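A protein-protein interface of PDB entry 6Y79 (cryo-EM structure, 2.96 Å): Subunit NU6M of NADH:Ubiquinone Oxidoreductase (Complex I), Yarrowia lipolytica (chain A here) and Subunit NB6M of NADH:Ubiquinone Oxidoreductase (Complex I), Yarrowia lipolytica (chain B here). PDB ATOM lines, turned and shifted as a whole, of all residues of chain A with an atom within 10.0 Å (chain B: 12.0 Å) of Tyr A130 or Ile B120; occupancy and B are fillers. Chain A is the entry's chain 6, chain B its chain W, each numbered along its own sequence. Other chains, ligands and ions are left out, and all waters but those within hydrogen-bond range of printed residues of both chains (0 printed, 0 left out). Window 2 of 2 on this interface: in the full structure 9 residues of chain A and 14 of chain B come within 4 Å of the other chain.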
ATOM      1  N   TYR A   6      33.767   0.808  26.236  1.00  0.00           N
ATOM      2  CA  TYR A   6      32.580   1.275  25.536  1.00  0.00           C
ATOM      3  C   TYR A   6      32.833   1.389  24.039  1.00  0.00           C
ATOM      4  O   TYR A   6      32.012   0.961  23.223  1.00  0.00           O
ATOM      5  CB  TYR A   6      32.161   2.625  26.124  1.00  0.00           C
ATOM      6  CG  TYR A   6      31.065   3.346  25.390  1.00  0.00           C
ATOM      7  CD1 TYR A   6      29.735   3.036  25.615  1.00  0.00           C
ATOM      8  CD2 TYR A   6      31.359   4.358  24.488  1.00  0.00           C
ATOM      9  CE1 TYR A   6      28.732   3.697  24.951  1.00  0.00           C
ATOM     10  CE2 TYR A   6      30.368   5.017  23.815  1.00  0.00           C
ATOM     11  CZ  TYR A   6      29.056   4.685  24.053  1.00  0.00           C
ATOM     12  OH  TYR A   6      28.060   5.347  23.388  1.00  0.00           O
ATOM     13  N   LEU A 123      20.934  12.516   7.822  1.00  0.00           N
ATOM     14  CA  LEU A 123      21.333  12.661   9.225  1.00  0.00           C
ATOM     15  C   LEU A 123      20.500  11.806  10.178  1.00  0.00           C
ATOM     16  O   LEU A 123      20.793  11.770  11.379  1.00  0.00           O
ATOM     17  CB  LEU A 123      21.291  14.138   9.632  1.00  0.00           C
ATOM     18  CG  LEU A 123      22.347  14.990   8.912  1.00  0.00           C
ATOM     19  CD1 LEU A 123      22.368  16.446   9.369  1.00  0.00           C
ATOM     20  CD2 LEU A 123      23.748  14.380   8.996  1.00  0.00           C
ATOM     21  N   GLU A 124      19.489  11.091   9.671  1.00  0.00           N
ATOM     22  CA  GLU A 124      18.897  10.012  10.453  1.00  0.00           C
ATOM     23  C   GLU A 124      19.802   8.792  10.511  1.00  0.00           C
ATOM     24  O   GLU A 124      19.571   7.904  11.338  1.00  0.00           O
ATOM     25  CB  GLU A 124      17.538   9.583   9.908  1.00  0.00           C
ATOM     26  CG  GLU A 124      16.384  10.506  10.217  1.00  0.00           C
ATOM     27  CD  GLU A 124      15.063   9.988   9.681  1.00  0.00           C
ATOM     28  OE1 GLU A 124      15.057   8.911   9.046  1.00  0.00           O
ATOM     29  OE2 GLU A 124      14.033  10.671   9.867  1.00  0.00           O
ATOM     30  N   PHE A 126      22.844   9.176  11.408  1.00  0.00           N
ATOM     31  CA  PHE A 126      23.668   9.518  12.559  1.00  0.00           C
ATOM     32  C   PHE A 126      22.871   9.678  13.842  1.00  0.00           C
ATOM     33  O   PHE A 126      23.474   9.849  14.907  1.00  0.00           O
ATOM     34  CB  PHE A 126      24.443  10.808  12.301  1.00  0.00           C
ATOM     35  CG  PHE A 126      25.451  10.696  11.201  1.00  0.00           C
ATOM     36  CD1 PHE A 126      26.675  10.088  11.416  1.00  0.00           C
ATOM     37  CD2 PHE A 126      25.166  11.204   9.946  1.00  0.00           C
ATOM     38  CE1 PHE A 126      27.607   9.992  10.393  1.00  0.00           C
ATOM     39  CE2 PHE A 126      26.088  11.111   8.921  1.00  0.00           C
ATOM     40  CZ  PHE A 126      27.304  10.507   9.152  1.00  0.00           C
ATOM     41  N   GLY A 127      21.543   9.610  13.775  1.00  0.00           N
ATOM     42  CA  GLY A 127      20.722   9.673  14.968  1.00  0.00           C
ATOM     43  C   GLY A 127      20.775   8.351  15.704  1.00  0.00           C
ATOM     44  O   GLY A 127      19.807   7.583  15.708  1.00  0.00           O
ATOM     45  N   ASN A 128      21.916   8.081  16.342  1.00  0.00           N
ATOM     46  CA  ASN A 128      22.234   6.758  16.843  1.00  0.00           C
ATOM     47  C   ASN A 128      22.156   6.650  18.355  1.00  0.00           C
ATOM     48  O   ASN A 128      22.007   5.541  18.870  1.00  0.00           O
ATOM     49  CB  ASN A 128      23.654   6.365  16.425  1.00  0.00           C
ATOM     50  CG  ASN A 128      23.804   6.209  14.939  1.00  0.00           C
ATOM     51  OD1 ASN A 128      22.977   5.579  14.278  1.00  0.00           O
ATOM     52  ND2 ASN A 128      24.862   6.793  14.394  1.00  0.00           N
ATOM     53  N   ASP A 129      22.211   7.763  19.071  1.00  0.00           N
ATOM     54  CA  ASP A 129      22.613   7.961  20.462  1.00  0.00           C
ATOM     55  C   ASP A 129      21.750   7.174  21.506  1.00  0.00           C
ATOM     56  O   ASP A 129      22.100   7.079  22.692  1.00  0.00           O
ATOM     57  CB  ASP A 129      22.563   9.466  20.723  1.00  0.00           C
ATOM     58  CG  ASP A 129      23.088   9.847  22.090  1.00  0.00           C
ATOM     59  OD1 ASP A 129      24.172   9.361  22.469  1.00  0.00           O
ATOM     60  OD2 ASP A 129      22.404  10.628  22.780  1.00  0.00           O
ATOM     61  N   TYR A 130      20.662   6.496  21.182  1.00  0.00           N
ATOM     62  CA  TYR A 130      19.753   6.025  22.212  1.00  0.00           C
ATOM     63  C   TYR A 130      20.022   4.563  22.529  1.00  0.00           C
ATOM     64  O   TYR A 130      20.223   3.748  21.625  1.00  0.00           O
ATOM     65  CB  TYR A 130      18.320   6.297  21.772  1.00  0.00           C
ATOM     66  CG  TYR A 130      18.148   7.789  21.734  1.00  0.00           C
ATOM     67  CD1 TYR A 130      17.995   8.501  22.910  1.00  0.00           C
ATOM     68  CD2 TYR A 130      18.241   8.495  20.541  1.00  0.00           C
ATOM     69  CE1 TYR A 130      17.884   9.860  22.901  1.00  0.00           C
ATOM     70  CE2 TYR A 130      18.136   9.857  20.522  1.00  0.00           C
ATOM     71  CZ  TYR A 130      17.958  10.533  21.707  1.00  0.00           C
ATOM     72  OH  TYR A 130      17.862  11.893  21.699  1.00  0.00           O
ATOM     73  N   ASN A 131      20.066   4.250  23.820  1.00  0.00           N
ATOM     74  CA  ASN A 131      20.571   2.973  24.308  1.00  0.00           C
ATOM     75  C   ASN A 131      19.409   2.000  24.434  1.00  0.00           C
ATOM     76  O   ASN A 131      18.493   2.237  25.224  1.00  0.00           O
ATOM     77  CB  ASN A 131      21.271   3.154  25.651  1.00  0.00           C
ATOM     78  CG  ASN A 131      22.732   3.461  25.504  1.00  0.00           C
ATOM     79  OD1 ASN A 131      23.190   3.841  24.433  1.00  0.00           O
ATOM     80  ND2 ASN A 131      23.483   3.279  26.579  1.00  0.00           N
ATOM     81  N   THR A 132      19.454   0.906  23.674  1.00  0.00           N
ATOM     82  CA  THR A 132      18.347  -0.042  23.641  1.00  0.00           C
ATOM     83  C   THR A 132      18.165  -0.723  24.994  1.00  0.00           C
ATOM     84  O   THR A 132      19.131  -1.028  25.693  1.00  0.00           O
ATOM     85  CB  THR A 132      18.550  -1.069  22.506  1.00  0.00           C
ATOM     86  OG1 THR A 132      17.437  -1.969  22.449  1.00  0.00           O
ATOM     87  CG2 THR A 132      19.847  -1.847  22.630  1.00  0.00           C
ATOM     88  N   ILE A 133      16.913  -0.863  25.405  1.00  0.00           N
ATOM     89  CA  ILE A 133      16.579  -1.477  26.683  1.00  0.00           C
ATOM     90  C   ILE A 133      16.346  -2.960  26.446  1.00  0.00           C
ATOM     91  O   ILE A 133      15.481  -3.339  25.650  1.00  0.00           O
ATOM     92  CB  ILE A 133      15.345  -0.819  27.316  1.00  0.00           C
ATOM     93  CG1 ILE A 133      15.665   0.609  27.745  1.00  0.00           C
ATOM     94  CG2 ILE A 133      14.860  -1.628  28.494  1.00  0.00           C
ATOM     95  CD1 ILE A 133      14.507   1.328  28.389  1.00  0.00           C
ATOM     96  N   ILE A 134      17.116  -3.802  27.127  1.00  0.00           N
ATOM     97  CA  ILE A 134      16.998  -5.248  27.003  1.00  0.00           C
ATOM     98  C   ILE A 134      16.188  -5.767  28.184  1.00  0.00           C
ATOM     99  O   ILE A 134      16.549  -5.542  29.343  1.00  0.00           O
ATOM    100  CB  ILE A 134      18.374  -5.923  26.932  1.00  0.00           C
ATOM    101  CG1 ILE A 134      19.109  -5.502  25.662  1.00  0.00           C
ATOM    102  CG2 ILE A 134      18.221  -7.421  26.954  1.00  0.00           C
ATOM    103  CD1 ILE A 134      18.381  -5.870  24.395  1.00  0.00           C
ATOM    104  N   ARG B  84       8.333  -0.349  36.301  1.00  0.00           N
ATOM    105  CA  ARG B  84       9.420   0.495  35.809  1.00  0.00           C
ATOM    106  C   ARG B  84       8.991   1.355  34.629  1.00  0.00           C
ATOM    107  O   ARG B  84       9.493   2.474  34.470  1.00  0.00           O
ATOM    108  CB  ARG B  84      10.612  -0.358  35.421  1.00  0.00           C
ATOM    109  CG  ARG B  84      11.143  -1.195  36.548  1.00  0.00           C
ATOM    110  CD  ARG B  84      12.218  -2.079  36.048  1.00  0.00           C
ATOM    111  NE  ARG B  84      13.257  -1.237  35.503  1.00  0.00           N
ATOM    112  CZ  ARG B  84      14.399  -1.001  36.121  1.00  0.00           C
ATOM    113  NH1 ARG B  84      15.299  -0.202  35.582  1.00  0.00           N
ATOM    114  NH2 ARG B  84      14.634  -1.578  37.282  1.00  0.00           N
ATOM    115  N   GLN B  88       9.069   5.390  34.555  1.00  0.00           N
ATOM    116  CA  GLN B  88       9.713   6.193  33.516  1.00  0.00           C
ATOM    117  C   GLN B  88       8.752   7.216  32.921  1.00  0.00           C
ATOM    118  O   GLN B  88       9.147   8.351  32.616  1.00  0.00           O
ATOM    119  CB  GLN B  88      10.258   5.280  32.421  1.00  0.00           C
ATOM    120  CG  GLN B  88      11.000   6.002  31.315  1.00  0.00           C
ATOM    121  CD  GLN B  88      12.341   6.515  31.771  1.00  0.00           C
ATOM    122  OE1 GLN B  88      13.074   5.821  32.474  1.00  0.00           O
ATOM    123  NE2 GLN B  88      12.672   7.738  31.385  1.00  0.00           N
ATOM    124  N   LEU B  89       7.483   6.825  32.767  1.00  0.00           N
ATOM    125  CA  LEU B  89       6.455   7.718  32.243  1.00  0.00           C
ATOM    126  C   LEU B  89       6.233   8.910  33.162  1.00  0.00           C
ATOM    127  O   LEU B  89       6.248  10.069  32.718  1.00  0.00           O
ATOM    128  CB  LEU B  89       5.158   6.937  32.065  1.00  0.00           C
ATOM    129  CG  LEU B  89       3.960   7.720  31.556  1.00  0.00           C
ATOM    130  CD1 LEU B  89       4.185   8.087  30.114  1.00  0.00           C
ATOM    131  CD2 LEU B  89       2.701   6.901  31.715  1.00  0.00           C
ATOM    132  N   ARG B  91       8.386   9.895  35.288  1.00  0.00           N
ATOM    133  CA  ARG B  91       9.653  10.611  35.363  1.00  0.00           C
ATOM    134  C   ARG B  91       9.750  11.666  34.273  1.00  0.00           C
ATOM    135  O   ARG B  91      10.060  12.825  34.556  1.00  0.00           O
ATOM    136  CB  ARG B  91      10.817   9.636  35.262  1.00  0.00           C
ATOM    137  CG  ARG B  91      12.184  10.294  35.389  1.00  0.00           C
ATOM    138  CD  ARG B  91      13.258   9.277  35.735  1.00  0.00           C
ATOM    139  NE  ARG B  91      12.719   8.157  36.502  1.00  0.00           N
ATOM    140  CZ  ARG B  91      12.698   6.899  36.073  1.00  0.00           C
ATOM    141  NH1 ARG B  91      12.180   5.947  36.834  1.00  0.00           N
ATOM    142  NH2 ARG B  91      13.164   6.607  34.871  1.00  0.00           N
ATOM    143  N   GLU B  92       9.444  11.301  33.021  1.00  0.00           N
ATOM    144  CA  GLU B  92       9.527  12.318  31.972  1.00  0.00           C
ATOM    145  C   GLU B  92       8.330  13.266  32.000  1.00  0.00           C
ATOM    146  O   GLU B  92       8.398  14.346  31.402  1.00  0.00           O
ATOM    147  CB  GLU B  92       9.693  11.681  30.596  1.00  0.00           C
ATOM    148  CG  GLU B  92       8.738  10.573  30.249  1.00  0.00           C
ATOM    149  CD  GLU B  92       9.373   9.580  29.299  1.00  0.00           C
ATOM    150  OE1 GLU B  92       8.653   8.744  28.721  1.00  0.00           O
ATOM    151  OE2 GLU B  92      10.613   9.628  29.142  1.00  0.00           O
ATOM    152  N   LYS B  93       7.235  12.903  32.686  1.00  0.00           N
ATOM    153  CA  LYS B  93       6.228  13.914  33.015  1.00  0.00           C
ATOM    154  C   LYS B  93       6.776  14.931  34.015  1.00  0.00           C
ATOM    155  O   LYS B  93       6.552  16.137  33.870  1.00  0.00           O
ATOM    156  CB  LYS B  93       4.974  13.245  33.557  1.00  0.00           C
ATOM    157  CG  LYS B  93       3.793  14.172  33.752  1.00  0.00           C
ATOM    158  CD  LYS B  93       2.610  13.412  34.323  1.00  0.00           C
ATOM    159  CE  LYS B  93       2.043  12.449  33.297  1.00  0.00           C
ATOM    160  NZ  LYS B  93       1.452  13.166  32.140  1.00  0.00           N
ATOM    161  N   ILE B  95       9.844  15.632  34.167  1.00  0.00           N
ATOM    162  CA  ILE B  95      10.880  16.377  33.458  1.00  0.00           C
ATOM    163  C   ILE B  95      10.269  17.560  32.716  1.00  0.00           C
ATOM    164  O   ILE B  95      10.692  18.702  32.897  1.00  0.00           O
ATOM    165  CB  ILE B  95      11.679  15.457  32.513  1.00  0.00           C
ATOM    166  CG1 ILE B  95      12.570  14.489  33.303  1.00  0.00           C
ATOM    167  CG2 ILE B  95      12.512  16.283  31.530  1.00  0.00           C
ATOM    168  CD1 ILE B  95      13.203  13.416  32.454  1.00  0.00           C
ATOM    169  N   MET B  96       9.253  17.313  31.891  1.00  0.00           N
ATOM    170  CA  MET B  96       8.724  18.324  30.981  1.00  0.00           C
ATOM    171  C   MET B  96       7.473  19.011  31.506  1.00  0.00           C
ATOM    172  O   MET B  96       6.556  19.300  30.726  1.00  0.00           O
ATOM    173  CB  MET B  96       8.456  17.705  29.617  1.00  0.00           C
ATOM    174  CG  MET B  96       9.612  16.899  29.131  1.00  0.00           C
ATOM    175  SD  MET B  96       9.398  16.592  27.389  1.00  0.00           S
ATOM    176  CE  MET B  96       9.301  18.256  26.745  1.00  0.00           C
ATOM    177  N   PHE B 101       3.778  19.457  26.357  1.00  0.00           N
ATOM    178  CA  PHE B 101       4.177  18.277  25.609  1.00  0.00           C
ATOM    179  C   PHE B 101       3.485  17.072  26.227  1.00  0.00           C
ATOM    180  O   PHE B 101       3.423  16.949  27.453  1.00  0.00           O
ATOM    181  CB  PHE B 101       5.698  18.093  25.631  1.00  0.00           C
ATOM    182  CG  PHE B 101       6.182  16.888  24.872  1.00  0.00           C
ATOM    183  CD1 PHE B 101       6.276  16.909  23.492  1.00  0.00           C
ATOM    184  CD2 PHE B 101       6.564  15.742  25.545  1.00  0.00           C
ATOM    185  CE1 PHE B 101       6.734  15.802  22.800  1.00  0.00           C
ATOM    186  CE2 PHE B 101       7.025  14.636  24.863  1.00  0.00           C
ATOM    187  CZ  PHE B 101       7.108  14.667  23.490  1.00  0.00           C
ATOM    188  N   VAL B 103       3.552  13.462  27.248  1.00  0.00           N
ATOM    189  CA  VAL B 103       4.404  12.297  27.451  1.00  0.00           C
ATOM    190  C   VAL B 103       3.580  11.018  27.601  1.00  0.00           C
ATOM    191  O   VAL B 103       4.107   9.919  27.388  1.00  0.00           O
ATOM    192  CB  VAL B 103       5.353  12.481  28.650  1.00  0.00           C
ATOM    193  CG1 VAL B 103       6.158  13.762  28.524  1.00  0.00           C
ATOM    194  CG2 VAL B 103       4.591  12.451  29.956  1.00  0.00           C
ATOM    195  N   PRO B 116       8.749   0.883  27.221  1.00  0.00           N
ATOM    196  CA  PRO B 116       9.615   1.821  26.509  1.00  0.00           C
ATOM    197  C   PRO B 116      10.974   1.204  26.236  1.00  0.00           C
ATOM    198  O   PRO B 116      11.399   0.242  26.878  1.00  0.00           O
ATOM    199  CB  PRO B 116       9.733   2.998  27.479  1.00  0.00           C
ATOM    200  CG  PRO B 116       9.621   2.360  28.810  1.00  0.00           C
ATOM    201  CD  PRO B 116       8.623   1.242  28.641  1.00  0.00           C
ATOM    202  N   ALA B 117      11.654   1.778  25.255  1.00  0.00           N
ATOM    203  CA  ALA B 117      13.012   1.388  24.928  1.00  0.00           C
ATOM    204  C   ALA B 117      13.815   2.649  24.650  1.00  0.00           C
ATOM    205  O   ALA B 117      13.321   3.770  24.804  1.00  0.00           O
ATOM    206  CB  ALA B 117      13.038   0.421  23.741  1.00  0.00           C
ATOM    207  N   LEU B 118      15.084   2.440  24.297  1.00  0.00           N
ATOM    208  CA  LEU B 118      15.945   3.445  23.673  1.00  0.00           C
ATOM    209  C   LEU B 118      16.240   4.619  24.610  1.00  0.00           C
ATOM    210  O   LEU B 118      16.199   5.778  24.205  1.00  0.00           O
ATOM    211  CB  LEU B 118      15.359   3.928  22.344  1.00  0.00           C
ATOM    212  CG  LEU B 118      15.756   3.168  21.080  1.00  0.00           C
ATOM    213  CD1 LEU B 118      15.245   1.752  21.052  1.00  0.00           C
ATOM    214  CD2 LEU B 118      15.209   3.913  19.916  1.00  0.00           C
ATOM    215  N   MET B 119      16.572   4.315  25.859  1.00  0.00           N
ATOM    216  CA  MET B 119      16.832   5.349  26.849  1.00  0.00           C
ATOM    217  C   MET B 119      18.153   6.063  26.581  1.00  0.00           C
ATOM    218  O   MET B 119      19.019   5.571  25.859  1.00  0.00           O
ATOM    219  CB  MET B 119      16.878   4.732  28.235  1.00  0.00           C
ATOM    220  CG  MET B 119      17.843   3.584  28.306  1.00  0.00           C
ATOM    221  SD  MET B 119      18.134   3.094  29.998  1.00  0.00           S
ATOM    222  CE  MET B 119      18.979   4.492  30.702  1.00  0.00           C
ATOM    223  N   ILE B 120      18.299   7.230  27.186  1.00  0.00           N
ATOM    224  CA  ILE B 120      19.546   7.999  27.100  1.00  0.00           C
ATOM    225  C   ILE B 120      20.577   7.376  28.030  1.00  0.00           C
ATOM    226  O   ILE B 120      20.230   7.014  29.164  1.00  0.00           O
ATOM    227  CB  ILE B 120      19.274   9.449  27.478  1.00  0.00           C
ATOM    228  CG1 ILE B 120      17.925   9.852  26.892  1.00  0.00           C
ATOM    229  CG2 ILE B 120      20.406  10.369  27.016  1.00  0.00           C
ATOM    230  CD1 ILE B 120      17.328  11.051  27.529  1.00  0.00           C
ATOM    231  N   PRO B 121      21.832   7.227  27.616  1.00  0.00           N
ATOM    232  CA  PRO B 121      22.849   6.651  28.506  1.00  0.00           C
ATOM    233  C   PRO B 121      23.160   7.568  29.678  1.00  0.00           C
ATOM    234  O   PRO B 121      23.262   8.793  29.519  1.00  0.00           O
ATOM    235  CB  PRO B 121      24.071   6.485  27.590  1.00  0.00           C
ATOM    236  CG  PRO B 121      23.802   7.361  26.422  1.00  0.00           C
ATOM    237  CD  PRO B 121      22.325   7.335  26.235  1.00  0.00           C
ATOM    238  N   PRO B 122      23.299   7.008  30.887  1.00  0.00           N
ATOM    239  CA  PRO B 122      23.609   7.747  32.115  1.00  0.00           C
ATOM    240  C   PRO B 122      25.105   8.005  32.295  1.00  0.00           C
ATOM    241  O   PRO B 122      25.481   8.969  32.964  1.00  0.00           O
ATOM    242  CB  PRO B 122      23.091   6.820  33.202  1.00  0.00           C
ATOM    243  CG  PRO B 122      23.274   5.483  32.607  1.00  0.00           C
ATOM    244  CD  PRO B 122      23.047   5.584  31.161  1.00  0.00           C
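The backbone NH (N) of Asn A131 is in hydrogen-bond range of the backbone carbonyl oxygen (O) of Met B119, at 2.6 Å.
Among the printed residues, pairs that only touch across the chains: Asp A129 with Pro B121 (3.6 Å), Tyr A130 with Leu B118 (3.3 Å), Tyr A130 with Met B119 (3.6 Å), Tyr A130 with Ile B120 (3.99 Å), Asn A131 with Leu B118 (3.2 Å), Asn A131 with Pro B121 (3.4 Å), Ile A133 with Pro B116 (3.6 Å), Ile A133 with Ala B117 (3.8 Å), Ile A133 with Leu B118 (3.9 Å) and Ile A133 with Met B119 (3.7 Å).
Printed residues of chain B within 4 Å of Tyr A130: Leu B118 (3.3 Å), Met B119 (3.6 Å) and Ile B120 (3.99 Å).
Printed residues of chain A within 4 Å of Ile B120: Tyr A130.
Of chain B, only Pro B121 (3.6 Å) comes within 4 Å of Asp A129.
Of chain B, only Leu B118, Met B119 and Pro B121 come within 4 Å of Asn A131.
No residue of chain B comes within 4 Å of Thr A132.
Leu B118 touches three residues of chain A.
Of the printed residues of chain A, Ala B117 touches Ile A133.
Of the printed residues of chain A, Pro B116 touches Ile A133.
Printed residues of chain B within 4 Å of Ile A133: Pro B116 (3.6 Å), Ala B117 (3.8 Å), Leu B118 (3.9 Å) and Met B119 (3.7 Å).
The nearest printed residue of chain B that does not touch Tyr A130 is Pro B121 (5.0 Å).
The nearest printed residue of chain A that does not touch Ile B120 is Asp A129 (4.7 Å).
The nearest printed residue of chain A that does not touch Pro B116 is Ile A134 (7.0 Å).
Printed residues of chain B that touch a printed residue of chain A: Pro B116, Ala B117, Leu B118, Met B119, Ile B120 and Pro B121.
Hydrophobic or aromatic side chains of chain B within 4 Å of the printed part of chain A: Leu B118, Met B119, Ile B120 and Pro B121.
Hydrophobic or aromatic side chains of chain A that line the printed part of chain B: Tyr A130 and Ile A133.
Among the printed residues, no Asp or Glu carboxylate lies within 4 Å of a Lys or Arg side-chain nitrogen of the other chain.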
